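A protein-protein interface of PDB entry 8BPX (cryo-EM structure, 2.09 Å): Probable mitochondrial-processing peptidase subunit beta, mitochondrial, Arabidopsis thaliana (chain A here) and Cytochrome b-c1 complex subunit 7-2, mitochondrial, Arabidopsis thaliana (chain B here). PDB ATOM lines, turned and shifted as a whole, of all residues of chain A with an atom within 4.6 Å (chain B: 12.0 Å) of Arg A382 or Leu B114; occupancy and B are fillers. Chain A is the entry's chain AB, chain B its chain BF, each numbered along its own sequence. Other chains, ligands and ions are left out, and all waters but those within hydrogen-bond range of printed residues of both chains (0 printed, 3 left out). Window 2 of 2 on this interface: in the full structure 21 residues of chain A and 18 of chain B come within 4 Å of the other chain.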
ATOM      1  N   ASP A 378       4.721 -17.448  15.728  1.00  0.00           N
ATOM      2  CA  ASP A 378       4.403 -18.119  16.984  1.00  0.00           C
ATOM      3  C   ASP A 378       2.917 -18.437  17.102  1.00  0.00           C
ATOM      4  O   ASP A 378       2.553 -19.467  17.679  1.00  0.00           O
ATOM      5  CB  ASP A 378       4.855 -17.264  18.164  1.00  0.00           C
ATOM      6  CG  ASP A 378       6.335 -17.389  18.442  1.00  0.00           C
ATOM      7  OD1 ASP A 378       6.877 -18.502  18.296  1.00  0.00           O
ATOM      8  OD2 ASP A 378       6.958 -16.375  18.814  1.00  0.00           O
ATOM      9  N   LEU A 379       2.046 -17.572  16.580  1.00  0.00           N
ATOM     10  CA  LEU A 379       0.612 -17.846  16.624  1.00  0.00           C
ATOM     11  C   LEU A 379       0.268 -19.099  15.824  1.00  0.00           C
ATOM     12  O   LEU A 379      -0.463 -19.978  16.300  1.00  0.00           O
ATOM     13  CB  LEU A 379      -0.163 -16.635  16.101  1.00  0.00           C
ATOM     14  CG  LEU A 379      -1.672 -16.804  15.920  1.00  0.00           C
ATOM     15  CD1 LEU A 379      -2.335 -17.069  17.259  1.00  0.00           C
ATOM     16  CD2 LEU A 379      -2.263 -15.575  15.258  1.00  0.00           C
ATOM     17  N   THR A 380       0.801 -19.198  14.604  1.00  0.00           N
ATOM     18  CA  THR A 380       0.593 -20.399  13.803  1.00  0.00           C
ATOM     19  C   THR A 380       1.180 -21.623  14.491  1.00  0.00           C
ATOM     20  O   THR A 380       0.588 -22.705  14.455  1.00  0.00           O
ATOM     21  CB  THR A 380       1.203 -20.223  12.413  1.00  0.00           C
ATOM     22  OG1 THR A 380       0.602 -19.101  11.762  1.00  0.00           O
ATOM     23  CG2 THR A 380       0.975 -21.469  11.567  1.00  0.00           C
ATOM     24  N   GLN A 381       2.342 -21.468  15.130  1.00  0.00           N
ATOM     25  CA  GLN A 381       2.938 -22.585  15.855  1.00  0.00           C
ATOM     26  C   GLN A 381       2.014 -23.070  16.963  1.00  0.00           C
ATOM     27  O   GLN A 381       1.774 -24.268  17.100  1.00  0.00           O
ATOM     28  CB  GLN A 381       4.292 -22.180  16.430  1.00  0.00           C
ATOM     29  CG  GLN A 381       5.453 -22.341  15.480  1.00  0.00           C
ATOM     30  CD  GLN A 381       6.758 -21.889  16.099  1.00  0.00           C
ATOM     31  OE1 GLN A 381       7.478 -22.682  16.700  1.00  0.00           O
ATOM     32  NE2 GLN A 381       7.063 -20.606  15.963  1.00  0.00           N
ATOM     33  N   ARG A 382       1.479 -22.145  17.761  1.00  0.00           N
ATOM     34  CA  ARG A 382       0.594 -22.532  18.855  1.00  0.00           C
ATOM     35  C   ARG A 382      -0.644 -23.246  18.325  1.00  0.00           C
ATOM     36  O   ARG A 382      -1.023 -24.321  18.818  1.00  0.00           O
ATOM     37  CB  ARG A 382       0.208 -21.295  19.666  1.00  0.00           C
ATOM     38  CG  ARG A 382       1.170 -20.969  20.792  1.00  0.00           C
ATOM     39  CD  ARG A 382       0.907 -19.598  21.387  1.00  0.00           C
ATOM     40  NE  ARG A 382       2.114 -18.976  21.915  1.00  0.00           N
ATOM     41  CZ  ARG A 382       2.744 -19.363  23.018  1.00  0.00           C
ATOM     42  NH1 ARG A 382       2.306 -20.377  23.744  1.00  0.00           N
ATOM     43  NH2 ARG A 382       3.840 -18.717  23.400  1.00  0.00           N
ATOM     44  N   VAL A 383      -1.252 -22.686  17.277  1.00  0.00           N
ATOM     45  CA  VAL A 383      -2.483 -23.253  16.734  1.00  0.00           C
ATOM     46  C   VAL A 383      -2.230 -24.643  16.162  1.00  0.00           C
ATOM     47  O   VAL A 383      -2.990 -25.583  16.418  1.00  0.00           O
ATOM     48  CB  VAL A 383      -3.087 -22.304  15.682  1.00  0.00           C
ATOM     49  CG1 VAL A 383      -4.165 -23.009  14.879  1.00  0.00           C
ATOM     50  CG2 VAL A 383      -3.639 -21.061  16.360  1.00  0.00           C
ATOM     51  N   ALA A 384      -1.151 -24.801  15.391  1.00  0.00           N
ATOM     52  CA  ALA A 384      -0.879 -26.086  14.755  1.00  0.00           C
ATOM     53  C   ALA A 384      -0.389 -27.126  15.753  1.00  0.00           C
ATOM     54  O   ALA A 384      -0.700 -28.312  15.608  1.00  0.00           O
ATOM     55  CB  ALA A 384       0.138 -25.914  13.627  1.00  0.00           C
ATOM     56  N   ILE A 385       0.381 -26.713  16.760  1.00  0.00           N
ATOM     57  CA  ILE A 385       0.923 -27.658  17.727  1.00  0.00           C
ATOM     58  C   ILE A 385      -0.176 -28.185  18.639  1.00  0.00           C
ATOM     59  O   ILE A 385      -0.157 -29.355  19.036  1.00  0.00           O
ATOM     60  CB  ILE A 385       2.072 -27.002  18.519  1.00  0.00           C
ATOM     61  CG1 ILE A 385       3.354 -27.007  17.684  1.00  0.00           C
ATOM     62  CG2 ILE A 385       2.310 -27.718  19.842  1.00  0.00           C
ATOM     63  CD1 ILE A 385       4.337 -25.928  18.056  1.00  0.00           C
ATOM     64  N   ASN A 386      -1.154 -27.347  18.988  1.00  0.00           N
ATOM     65  CA  ASN A 386      -2.188 -27.807  19.903  1.00  0.00           C
ATOM     66  C   ASN A 386      -3.513 -28.157  19.226  1.00  0.00           C
ATOM     67  O   ASN A 386      -4.456 -28.542  19.923  1.00  0.00           O
ATOM     68  CB  ASN A 386      -2.405 -26.769  21.002  1.00  0.00           C
ATOM     69  CG  ASN A 386      -1.128 -26.466  21.763  1.00  0.00           C
ATOM     70  OD1 ASN A 386      -0.842 -27.087  22.780  1.00  0.00           O
ATOM     71  ND2 ASN A 386      -0.357 -25.506  21.274  1.00  0.00           N
ATOM     72  N   ILE A 388      -5.984 -26.341  17.659  1.00  0.00           N
ATOM     73  CA  ILE A 388      -7.022 -25.548  18.302  1.00  0.00           C
ATOM     74  C   ILE A 388      -7.779 -24.676  17.301  1.00  0.00           C
ATOM     75  O   ILE A 388      -8.456 -23.738  17.693  1.00  0.00           O
ATOM     76  CB  ILE A 388      -6.441 -24.704  19.452  1.00  0.00           C
ATOM     77  CG1 ILE A 388      -5.295 -23.826  18.950  1.00  0.00           C
ATOM     78  CG2 ILE A 388      -5.985 -25.599  20.591  1.00  0.00           C
ATOM     79  CD1 ILE A 388      -4.790 -22.846  19.976  1.00  0.00           C
ATOM     80  N   ALA A 422      -4.669 -17.624  22.760  1.00  0.00           N
ATOM     81  CA  ALA A 422      -3.462 -17.635  21.934  1.00  0.00           C
ATOM     82  C   ALA A 422      -3.412 -16.435  20.997  1.00  0.00           C
ATOM     83  O   ALA A 422      -2.363 -15.792  20.853  1.00  0.00           O
ATOM     84  CB  ALA A 422      -3.379 -18.936  21.137  1.00  0.00           C
ATOM     85  N   TYR A 425      -2.707 -13.290  23.034  1.00  0.00           N
ATOM     86  CA  TYR A 425      -1.337 -13.324  23.530  1.00  0.00           C
ATOM     87  C   TYR A 425      -0.350 -12.943  22.438  1.00  0.00           C
ATOM     88  O   TYR A 425       0.506 -12.075  22.637  1.00  0.00           O
ATOM     89  CB  TYR A 425      -1.007 -14.710  24.085  1.00  0.00           C
ATOM     90  CG  TYR A 425       0.353 -14.795  24.742  1.00  0.00           C
ATOM     91  CD1 TYR A 425       0.522 -14.460  26.078  1.00  0.00           C
ATOM     92  CD2 TYR A 425       1.470 -15.204  24.023  1.00  0.00           C
ATOM     93  CE1 TYR A 425       1.765 -14.534  26.682  1.00  0.00           C
ATOM     94  CE2 TYR A 425       2.717 -15.275  24.618  1.00  0.00           C
ATOM     95  CZ  TYR A 425       2.857 -14.941  25.947  1.00  0.00           C
ATOM     96  OH  TYR A 425       4.092 -15.013  26.540  1.00  0.00           O
ATOM     97  N   GLU A 426      -0.470 -13.565  21.262  1.00  0.00           N
ATOM     98  CA  GLU A 426       0.518 -13.319  20.220  1.00  0.00           C
ATOM     99  C   GLU A 426       0.356 -11.940  19.593  1.00  0.00           C
ATOM    100  O   GLU A 426       1.344 -11.356  19.137  1.00  0.00           O
ATOM    101  CB  GLU A 426       0.461 -14.414  19.155  1.00  0.00           C
ATOM    102  CG  GLU A 426       0.952 -15.780  19.638  1.00  0.00           C
ATOM    103  CD  GLU A 426       2.419 -15.795  20.067  1.00  0.00           C
ATOM    104  OE1 GLU A 426       3.161 -14.837  19.766  1.00  0.00           O
ATOM    105  OE2 GLU A 426       2.835 -16.780  20.705  1.00  0.00           O
ATOM    106  N   ASP B  46      10.601 -35.255  27.474  1.00  0.00           N
ATOM    107  CA  ASP B  46      11.475 -35.818  26.451  1.00  0.00           C
ATOM    108  C   ASP B  46      11.378 -37.337  26.426  1.00  0.00           C
ATOM    109  O   ASP B  46      11.300 -37.945  25.353  1.00  0.00           O
ATOM    110  CB  ASP B  46      12.917 -35.370  26.681  1.00  0.00           C
ATOM    111  CG  ASP B  46      13.110 -33.886  26.447  1.00  0.00           C
ATOM    112  OD1 ASP B  46      12.768 -33.401  25.347  1.00  0.00           O
ATOM    113  OD2 ASP B  46      13.610 -33.199  27.364  1.00  0.00           O
ATOM    114  N   GLU B  49       7.988 -38.278  24.892  1.00  0.00           N
ATOM    115  CA  GLU B  49       8.014 -38.139  23.439  1.00  0.00           C
ATOM    116  C   GLU B  49       8.797 -39.276  22.786  1.00  0.00           C
ATOM    117  O   GLU B  49       8.355 -39.852  21.781  1.00  0.00           O
ATOM    118  CB  GLU B  49       8.616 -36.784  23.066  1.00  0.00           C
ATOM    119  CG  GLU B  49       8.860 -36.593  21.583  1.00  0.00           C
ATOM    120  CD  GLU B  49       7.569 -36.487  20.791  1.00  0.00           C
ATOM    121  OE1 GLU B  49       6.514 -36.220  21.400  1.00  0.00           O
ATOM    122  OE2 GLU B  49       7.606 -36.677  19.558  1.00  0.00           O
ATOM    123  N   ARG B  53       7.455 -42.238  20.225  1.00  0.00           N
ATOM    124  CA  ARG B  53       8.007 -42.492  18.900  1.00  0.00           C
ATOM    125  C   ARG B  53       8.459 -43.934  18.693  1.00  0.00           C
ATOM    126  O   ARG B  53       8.813 -44.296  17.567  1.00  0.00           O
ATOM    127  CB  ARG B  53       9.168 -41.539  18.627  1.00  0.00           C
ATOM    128  CG  ARG B  53       8.699 -40.171  18.208  1.00  0.00           C
ATOM    129  CD  ARG B  53       9.831 -39.209  17.970  1.00  0.00           C
ATOM    130  NE  ARG B  53       9.337 -37.841  18.009  1.00  0.00           N
ATOM    131  CZ  ARG B  53      10.051 -36.770  17.696  1.00  0.00           C
ATOM    132  NH1 ARG B  53      11.313 -36.867  17.318  1.00  0.00           N
ATOM    133  NH2 ARG B  53       9.482 -35.571  17.761  1.00  0.00           N
ATOM    134  N   VAL B 101      15.512 -37.022  20.264  1.00  0.00           N
ATOM    135  CA  VAL B 101      14.503 -36.069  20.718  1.00  0.00           C
ATOM    136  C   VAL B 101      15.167 -34.862  21.369  1.00  0.00           C
ATOM    137  O   VAL B 101      14.759 -33.714  21.148  1.00  0.00           O
ATOM    138  CB  VAL B 101      13.506 -36.763  21.670  1.00  0.00           C
ATOM    139  CG1 VAL B 101      12.830 -35.752  22.578  1.00  0.00           C
ATOM    140  CG2 VAL B 101      12.471 -37.536  20.876  1.00  0.00           C
ATOM    141  N   LYS B 102      16.205 -35.100  22.176  1.00  0.00           N
ATOM    142  CA  LYS B 102      16.953 -33.999  22.778  1.00  0.00           C
ATOM    143  C   LYS B 102      17.591 -33.113  21.713  1.00  0.00           C
ATOM    144  O   LYS B 102      17.582 -31.882  21.831  1.00  0.00           O
ATOM    145  CB  LYS B 102      18.021 -34.541  23.730  1.00  0.00           C
ATOM    146  CG  LYS B 102      17.541 -34.800  25.147  1.00  0.00           C
ATOM    147  CD  LYS B 102      17.853 -36.216  25.607  1.00  0.00           C
ATOM    148  CE  LYS B 102      19.333 -36.540  25.471  1.00  0.00           C
ATOM    149  NZ  LYS B 102      19.638 -37.947  25.847  1.00  0.00           N
ATOM    150  N   ARG B 103      18.164 -33.725  20.674  1.00  0.00           N
ATOM    151  CA  ARG B 103      18.775 -32.951  19.599  1.00  0.00           C
ATOM    152  C   ARG B 103      17.741 -32.087  18.882  1.00  0.00           C
ATOM    153  O   ARG B 103      17.992 -30.911  18.593  1.00  0.00           O
ATOM    154  CB  ARG B 103      19.468 -33.890  18.612  1.00  0.00           C
ATOM    155  CG  ARG B 103      20.971 -33.696  18.495  1.00  0.00           C
ATOM    156  CD  ARG B 103      21.718 -35.031  18.429  1.00  0.00           C
ATOM    157  NE  ARG B 103      21.082 -35.982  17.524  1.00  0.00           N
ATOM    158  CZ  ARG B 103      20.957 -37.280  17.764  1.00  0.00           C
ATOM    159  NH1 ARG B 103      21.438 -37.829  18.867  1.00  0.00           N
ATOM    160  NH2 ARG B 103      20.332 -38.048  16.876  1.00  0.00           N
ATOM    161  N   GLU B 104      16.569 -32.657  18.589  1.00  0.00           N
ATOM    162  CA  GLU B 104      15.516 -31.885  17.931  1.00  0.00           C
ATOM    163  C   GLU B 104      15.035 -30.739  18.817  1.00  0.00           C
ATOM    164  O   GLU B 104      14.784 -29.629  18.332  1.00  0.00           O
ATOM    165  CB  GLU B 104      14.355 -32.801  17.547  1.00  0.00           C
ATOM    166  CG  GLU B 104      14.577 -33.535  16.239  1.00  0.00           C
ATOM    167  CD  GLU B 104      13.509 -34.571  15.954  1.00  0.00           C
ATOM    168  OE1 GLU B 104      12.438 -34.514  16.589  1.00  0.00           O
ATOM    169  OE2 GLU B 104      13.741 -35.438  15.085  1.00  0.00           O
ATOM    170  N   ARG B 105      14.938 -31.011  20.123  1.00  0.00           N
ATOM    171  CA  ARG B 105      14.525 -29.970  21.102  1.00  0.00           C
ATOM    172  C   ARG B 105      15.538 -28.825  21.072  1.00  0.00           C
ATOM    173  O   ARG B 105      15.106 -27.659  21.012  1.00  0.00           O
ATOM    174  CB  ARG B 105      14.483 -30.590  22.501  1.00  0.00           C
ATOM    175  CG  ARG B 105      13.956 -29.670  23.591  1.00  0.00           C
ATOM    176  CD  ARG B 105      12.443 -29.645  23.564  1.00  0.00           C
ATOM    177  NE  ARG B 105      11.863 -28.909  24.675  1.00  0.00           N
ATOM    178  CZ  ARG B 105      10.559 -28.757  24.874  1.00  0.00           C
ATOM    179  NH1 ARG B 105       9.692 -29.299  24.038  1.00  0.00           N
ATOM    180  NH2 ARG B 105      10.128 -28.078  25.922  1.00  0.00           N
ATOM    181  N   ALA B 106      16.834 -29.150  21.114  1.00  0.00           N
ATOM    182  CA  ALA B 106      17.875 -28.127  21.121  1.00  0.00           C
ATOM    183  C   ALA B 106      17.872 -27.329  19.823  1.00  0.00           C
ATOM    184  O   ALA B 106      18.078 -26.110  19.836  1.00  0.00           O
ATOM    185  CB  ALA B 106      19.244 -28.768  21.358  1.00  0.00           C
ATOM    186  N   GLU B 107      17.651 -28.001  18.692  1.00  0.00           N
ATOM    187  CA  GLU B 107      17.578 -27.294  17.417  1.00  0.00           C
ATOM    188  C   GLU B 107      16.401 -26.326  17.395  1.00  0.00           C
ATOM    189  O   GLU B 107      16.525 -25.198  16.905  1.00  0.00           O
ATOM    190  CB  GLU B 107      17.483 -28.299  16.267  1.00  0.00           C
ATOM    191  CG  GLU B 107      17.150 -27.686  14.917  1.00  0.00           C
ATOM    192  CD  GLU B 107      16.810 -28.730  13.868  1.00  0.00           C
ATOM    193  OE1 GLU B 107      15.821 -29.468  14.057  1.00  0.00           O
ATOM    194  OE2 GLU B 107      17.527 -28.813  12.851  1.00  0.00           O
ATOM    195  N   ARG B 108      15.253 -26.745  17.934  1.00  0.00           N
ATOM    196  CA  ARG B 108      14.118 -25.833  18.047  1.00  0.00           C
ATOM    197  C   ARG B 108      14.456 -24.631  18.920  1.00  0.00           C
ATOM    198  O   ARG B 108      14.108 -23.493  18.585  1.00  0.00           O
ATOM    199  CB  ARG B 108      12.905 -26.570  18.612  1.00  0.00           C
ATOM    200  CG  ARG B 108      12.130 -27.376  17.604  1.00  0.00           C
ATOM    201  CD  ARG B 108      10.804 -27.812  18.188  1.00  0.00           C
ATOM    202  NE  ARG B 108       9.765 -26.816  17.965  1.00  0.00           N
ATOM    203  CZ  ARG B 108       9.107 -26.667  16.825  1.00  0.00           C
ATOM    204  NH1 ARG B 108       9.365 -27.427  15.777  1.00  0.00           N
ATOM    205  NH2 ARG B 108       8.165 -25.736  16.736  1.00  0.00           N
ATOM    206  N   GLU B 109      15.128 -24.863  20.049  1.00  0.00           N
ATOM    207  CA  GLU B 109      15.467 -23.758  20.943  1.00  0.00           C
ATOM    208  C   GLU B 109      16.444 -22.785  20.291  1.00  0.00           C
ATOM    209  O   GLU B 109      16.326 -21.568  20.469  1.00  0.00           O
ATOM    210  CB  GLU B 109      16.040 -24.293  22.254  1.00  0.00           C
ATOM    211  CG  GLU B 109      15.001 -24.800  23.230  1.00  0.00           C
ATOM    212  CD  GLU B 109      14.417 -23.698  24.094  1.00  0.00           C
ATOM    213  OE1 GLU B 109      14.878 -22.542  23.982  1.00  0.00           O
ATOM    214  OE2 GLU B 109      13.499 -23.989  24.887  1.00  0.00           O
ATOM    215  N   ALA B 110      17.411 -23.298  19.527  1.00  0.00           N
ATOM    216  CA  ALA B 110      18.432 -22.434  18.939  1.00  0.00           C
ATOM    217  C   ALA B 110      17.858 -21.481  17.898  1.00  0.00           C
ATOM    218  O   ALA B 110      18.363 -20.367  17.737  1.00  0.00           O
ATOM    219  CB  ALA B 110      19.541 -23.279  18.317  1.00  0.00           C
ATOM    220  N   LEU B 111      16.816 -21.892  17.182  1.00  0.00           N
ATOM    221  CA  LEU B 111      16.236 -21.076  16.127  1.00  0.00           C
ATOM    222  C   LEU B 111      15.074 -20.217  16.607  1.00  0.00           C
ATOM    223  O   LEU B 111      14.433 -19.552  15.792  1.00  0.00           O
ATOM    224  CB  LEU B 111      15.793 -21.964  14.966  1.00  0.00           C
ATOM    225  CG  LEU B 111      16.961 -22.438  14.101  1.00  0.00           C
ATOM    226  CD1 LEU B 111      16.486 -23.369  13.002  1.00  0.00           C
ATOM    227  CD2 LEU B 111      17.692 -21.245  13.521  1.00  0.00           C
ATOM    228  N   GLY B 112      14.793 -20.215  17.907  1.00  0.00           N
ATOM    229  CA  GLY B 112      13.761 -19.360  18.453  1.00  0.00           C
ATOM    230  C   GLY B 112      12.343 -19.850  18.279  1.00  0.00           C
ATOM    231  O   GLY B 112      11.418 -19.035  18.307  1.00  0.00           O
ATOM    232  N   ALA B 113      12.140 -21.150  18.099  1.00  0.00           N
ATOM    233  CA  ALA B 113      10.808 -21.712  17.944  1.00  0.00           C
ATOM    234  C   ALA B 113      10.224 -22.118  19.293  1.00  0.00           C
ATOM    235  O   ALA B 113      10.943 -22.360  20.265  1.00  0.00           O
ATOM    236  CB  ALA B 113      10.831 -22.919  17.005  1.00  0.00           C
ATOM    237  N   LEU B 114       8.897 -22.188  19.334  1.00  0.00           N
ATOM    238  CA  LEU B 114       8.201 -22.638  20.527  1.00  0.00           C
ATOM    239  C   LEU B 114       8.440 -24.130  20.759  1.00  0.00           C
ATOM    240  O   LEU B 114       8.628 -24.891  19.808  1.00  0.00           O
ATOM    241  CB  LEU B 114       6.703 -22.374  20.402  1.00  0.00           C
ATOM    242  CG  LEU B 114       6.271 -20.911  20.347  1.00  0.00           C
ATOM    243  CD1 LEU B 114       4.771 -20.800  20.118  1.00  0.00           C
ATOM    244  CD2 LEU B 114       6.681 -20.183  21.613  1.00  0.00           C
ATOM    245  N   PRO B 115       8.445 -24.570  22.017  1.00  0.00           N
ATOM    246  CA  PRO B 115       8.580 -26.005  22.293  1.00  0.00           C
ATOM    247  C   PRO B 115       7.384 -26.783  21.765  1.00  0.00           C
ATOM    248  O   PRO B 115       6.259 -26.286  21.731  1.00  0.00           O
ATOM    249  CB  PRO B 115       8.652 -26.073  23.824  1.00  0.00           C
ATOM    250  CG  PRO B 115       8.920 -24.687  24.277  1.00  0.00           C
ATOM    251  CD  PRO B 115       8.349 -23.774  23.250  1.00  0.00           C
ATOM    252  N   LEU B 116       7.643 -28.022  21.349  1.00  0.00           N
ATOM    253  CA  LEU B 116       6.582 -28.893  20.863  1.00  0.00           C
ATOM    254  C   LEU B 116       5.737 -29.476  21.986  1.00  0.00           C
ATOM    255  O   LEU B 116       4.676 -30.041  21.710  1.00  0.00           O
ATOM    256  CB  LEU B 116       7.171 -30.029  20.026  1.00  0.00           C
ATOM    257  CG  LEU B 116       7.683 -29.679  18.629  1.00  0.00           C
ATOM    258  CD1 LEU B 116       8.251 -30.915  17.951  1.00  0.00           C
ATOM    259  CD2 LEU B 116       6.592 -29.043  17.777  1.00  0.00           C
ATOM    260  N   TYR B 117       6.188 -29.359  23.232  1.00  0.00           N
ATOM    261  CA  TYR B 117       5.457 -29.851  24.389  1.00  0.00           C
ATOM    262  C   TYR B 117       6.081 -29.236  25.633  1.00  0.00           C
ATOM    263  O   TYR B 117       7.264 -28.894  25.646  1.00  0.00           O
ATOM    264  CB  TYR B 117       5.478 -31.383  24.460  1.00  0.00           C
ATOM    265  CG  TYR B 117       6.836 -31.972  24.166  1.00  0.00           C
ATOM    266  CD1 TYR B 117       7.813 -32.037  25.148  1.00  0.00           C
ATOM    267  CD2 TYR B 117       7.146 -32.448  22.902  1.00  0.00           C
ATOM    268  CE1 TYR B 117       9.056 -32.565  24.884  1.00  0.00           C
ATOM    269  CE2 TYR B 117       8.388 -32.979  22.626  1.00  0.00           C
ATOM    270  CZ  TYR B 117       9.340 -33.034  23.621  1.00  0.00           C
ATOM    271  OH  TYR B 117      10.576 -33.562  23.354  1.00  0.00           O
ATOM    272  N   GLN B 118       5.316 -29.143  26.682  1.00  0.00           N
ATOM    273  CA  GLN B 118       5.786 -28.489  27.900  1.00  0.00           C
ATOM    274  C   GLN B 118       5.157 -29.254  29.042  1.00  0.00           C
ATOM    275  O   GLN B 118       4.099 -29.837  28.854  1.00  0.00           O
ATOM    276  CB  GLN B 118       5.558 -26.973  28.041  1.00  0.00           C
ATOM    277  CG  GLN B 118       6.015 -26.056  26.938  1.00  0.00           C
ATOM    278  CD  GLN B 118       5.338 -24.725  27.147  1.00  0.00           C
ATOM    279  OE1 GLN B 118       4.138 -24.587  26.953  1.00  0.00           O
ATOM    280  NE2 GLN B 118       6.096 -23.731  27.554  1.00  0.00           N
ATOM    281  N   ARG B 119       5.817 -29.171  30.205  1.00  0.00           N
ATOM    282  CA  ARG B 119       5.320 -29.830  31.434  1.00  0.00           C
ATOM    283  C   ARG B 119       4.254 -28.954  32.083  1.00  0.00           C
ATOM    284  O   ARG B 119       4.393 -27.713  32.040  1.00  0.00           O
ATOM    285  CB  ARG B 119       6.471 -30.003  32.430  1.00  0.00           C
ATOM    286  CG  ARG B 119       6.103 -30.781  33.685  1.00  0.00           C
ATOM    287  CD  ARG B 119       6.835 -30.294  34.919  1.00  0.00           C
ATOM    288  NE  ARG B 119       6.275 -30.876  36.130  1.00  0.00           N
ATOM    289  CZ  ARG B 119       6.664 -30.575  37.364  1.00  0.00           C
ATOM    290  NH1 ARG B 119       7.622 -29.685  37.562  1.00  0.00           N
ATOM    291  NH2 ARG B 119       6.089 -31.162  38.398  1.00  0.00           N
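The backbone carbonyl oxygen (O) of Arg A382 sits at hydrogen-bond distance from the side-chain amide nitrogen (ND2) of Asn A386. The backbone carbonyl oxygen (O) of Arg B108 sits at hydrogen-bond distance from the backbone NH (N) of Ala B113. The guanidinium group (NE) of Arg A382 is in salt-bridge range of the side-chain carboxylate (OE2) of Glu A426 (2.6 Å). The side-chain carboxylate of Asp A378 sits at hydrogen-bond distance from the side-chain amide nitrogen of Gln A381 (3.1 Å). NE of Arg B108 lies within hydrogen-bond range of O of Leu B114, 2.9 Å away.
Among the printed residues, merely in contact across the chains: Asp A378 with Leu B114, Gln A381 with Ala B113, Arg A382 with Leu B114 and Ile A385 with Leu B116.
Hydrophobic or aromatic side chains of chain B that line the printed part of chain A: Ala B113, Leu B114 and Leu B116. Of the 13 printed residues of chain A, 4 touch a printed residue of chain B. Printed residues of chain A that touch a printed residue of chain B: Asp A378, Gln A381, Arg A382 and Ile A385.
OE1 of Gln A381 is in hydrogen-bond range of NH2 of Arg B108 (3.1 Å). The backbone NH (N) of Leu B114 sits at hydrogen-bond distance from the side-chain amide oxygen (OE1) of Gln A381 (3.0 Å).
No residue of chain B comes within 4 Å of Leu A379. Thr A380 touches none of the printed residues of chain B. Gln A381 touches just these residues of chain B: Arg B108, Ala B113 and Leu B114. Of chain B, only Leu B114 comes within 4 Å of Arg A382. No residue of chain B comes within 4 Å of Val A383. Ala A384 touches none of the printed residues of chain B. Ile A385 touches just one residue of chain B: Leu B116. No residue of chain B comes within 4 Å of Asn A386. No residue of chain B comes within 4 Å of Ile A388. Ala A422 touches none of the printed residues of chain B. No residue of chain B comes within 4 Å of Tyr A425. Of the printed residues of chain A, Ala B113 touches Gln A381 (3.4 Å). Of the printed residues of chain A, Leu B114 touches Asp A378, Gln A381 and Arg A382. Of the printed residues of chain A, Leu B116 touches Ile A385. Gln B118 touches none of the printed residues of chain A. The nearest residue of chain A that does not touch Leu B114 is Glu A426 (4.5 Å). The nearest printed residue of chain A that does not touch Arg B108 is Ile A385 (4.1 Å).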
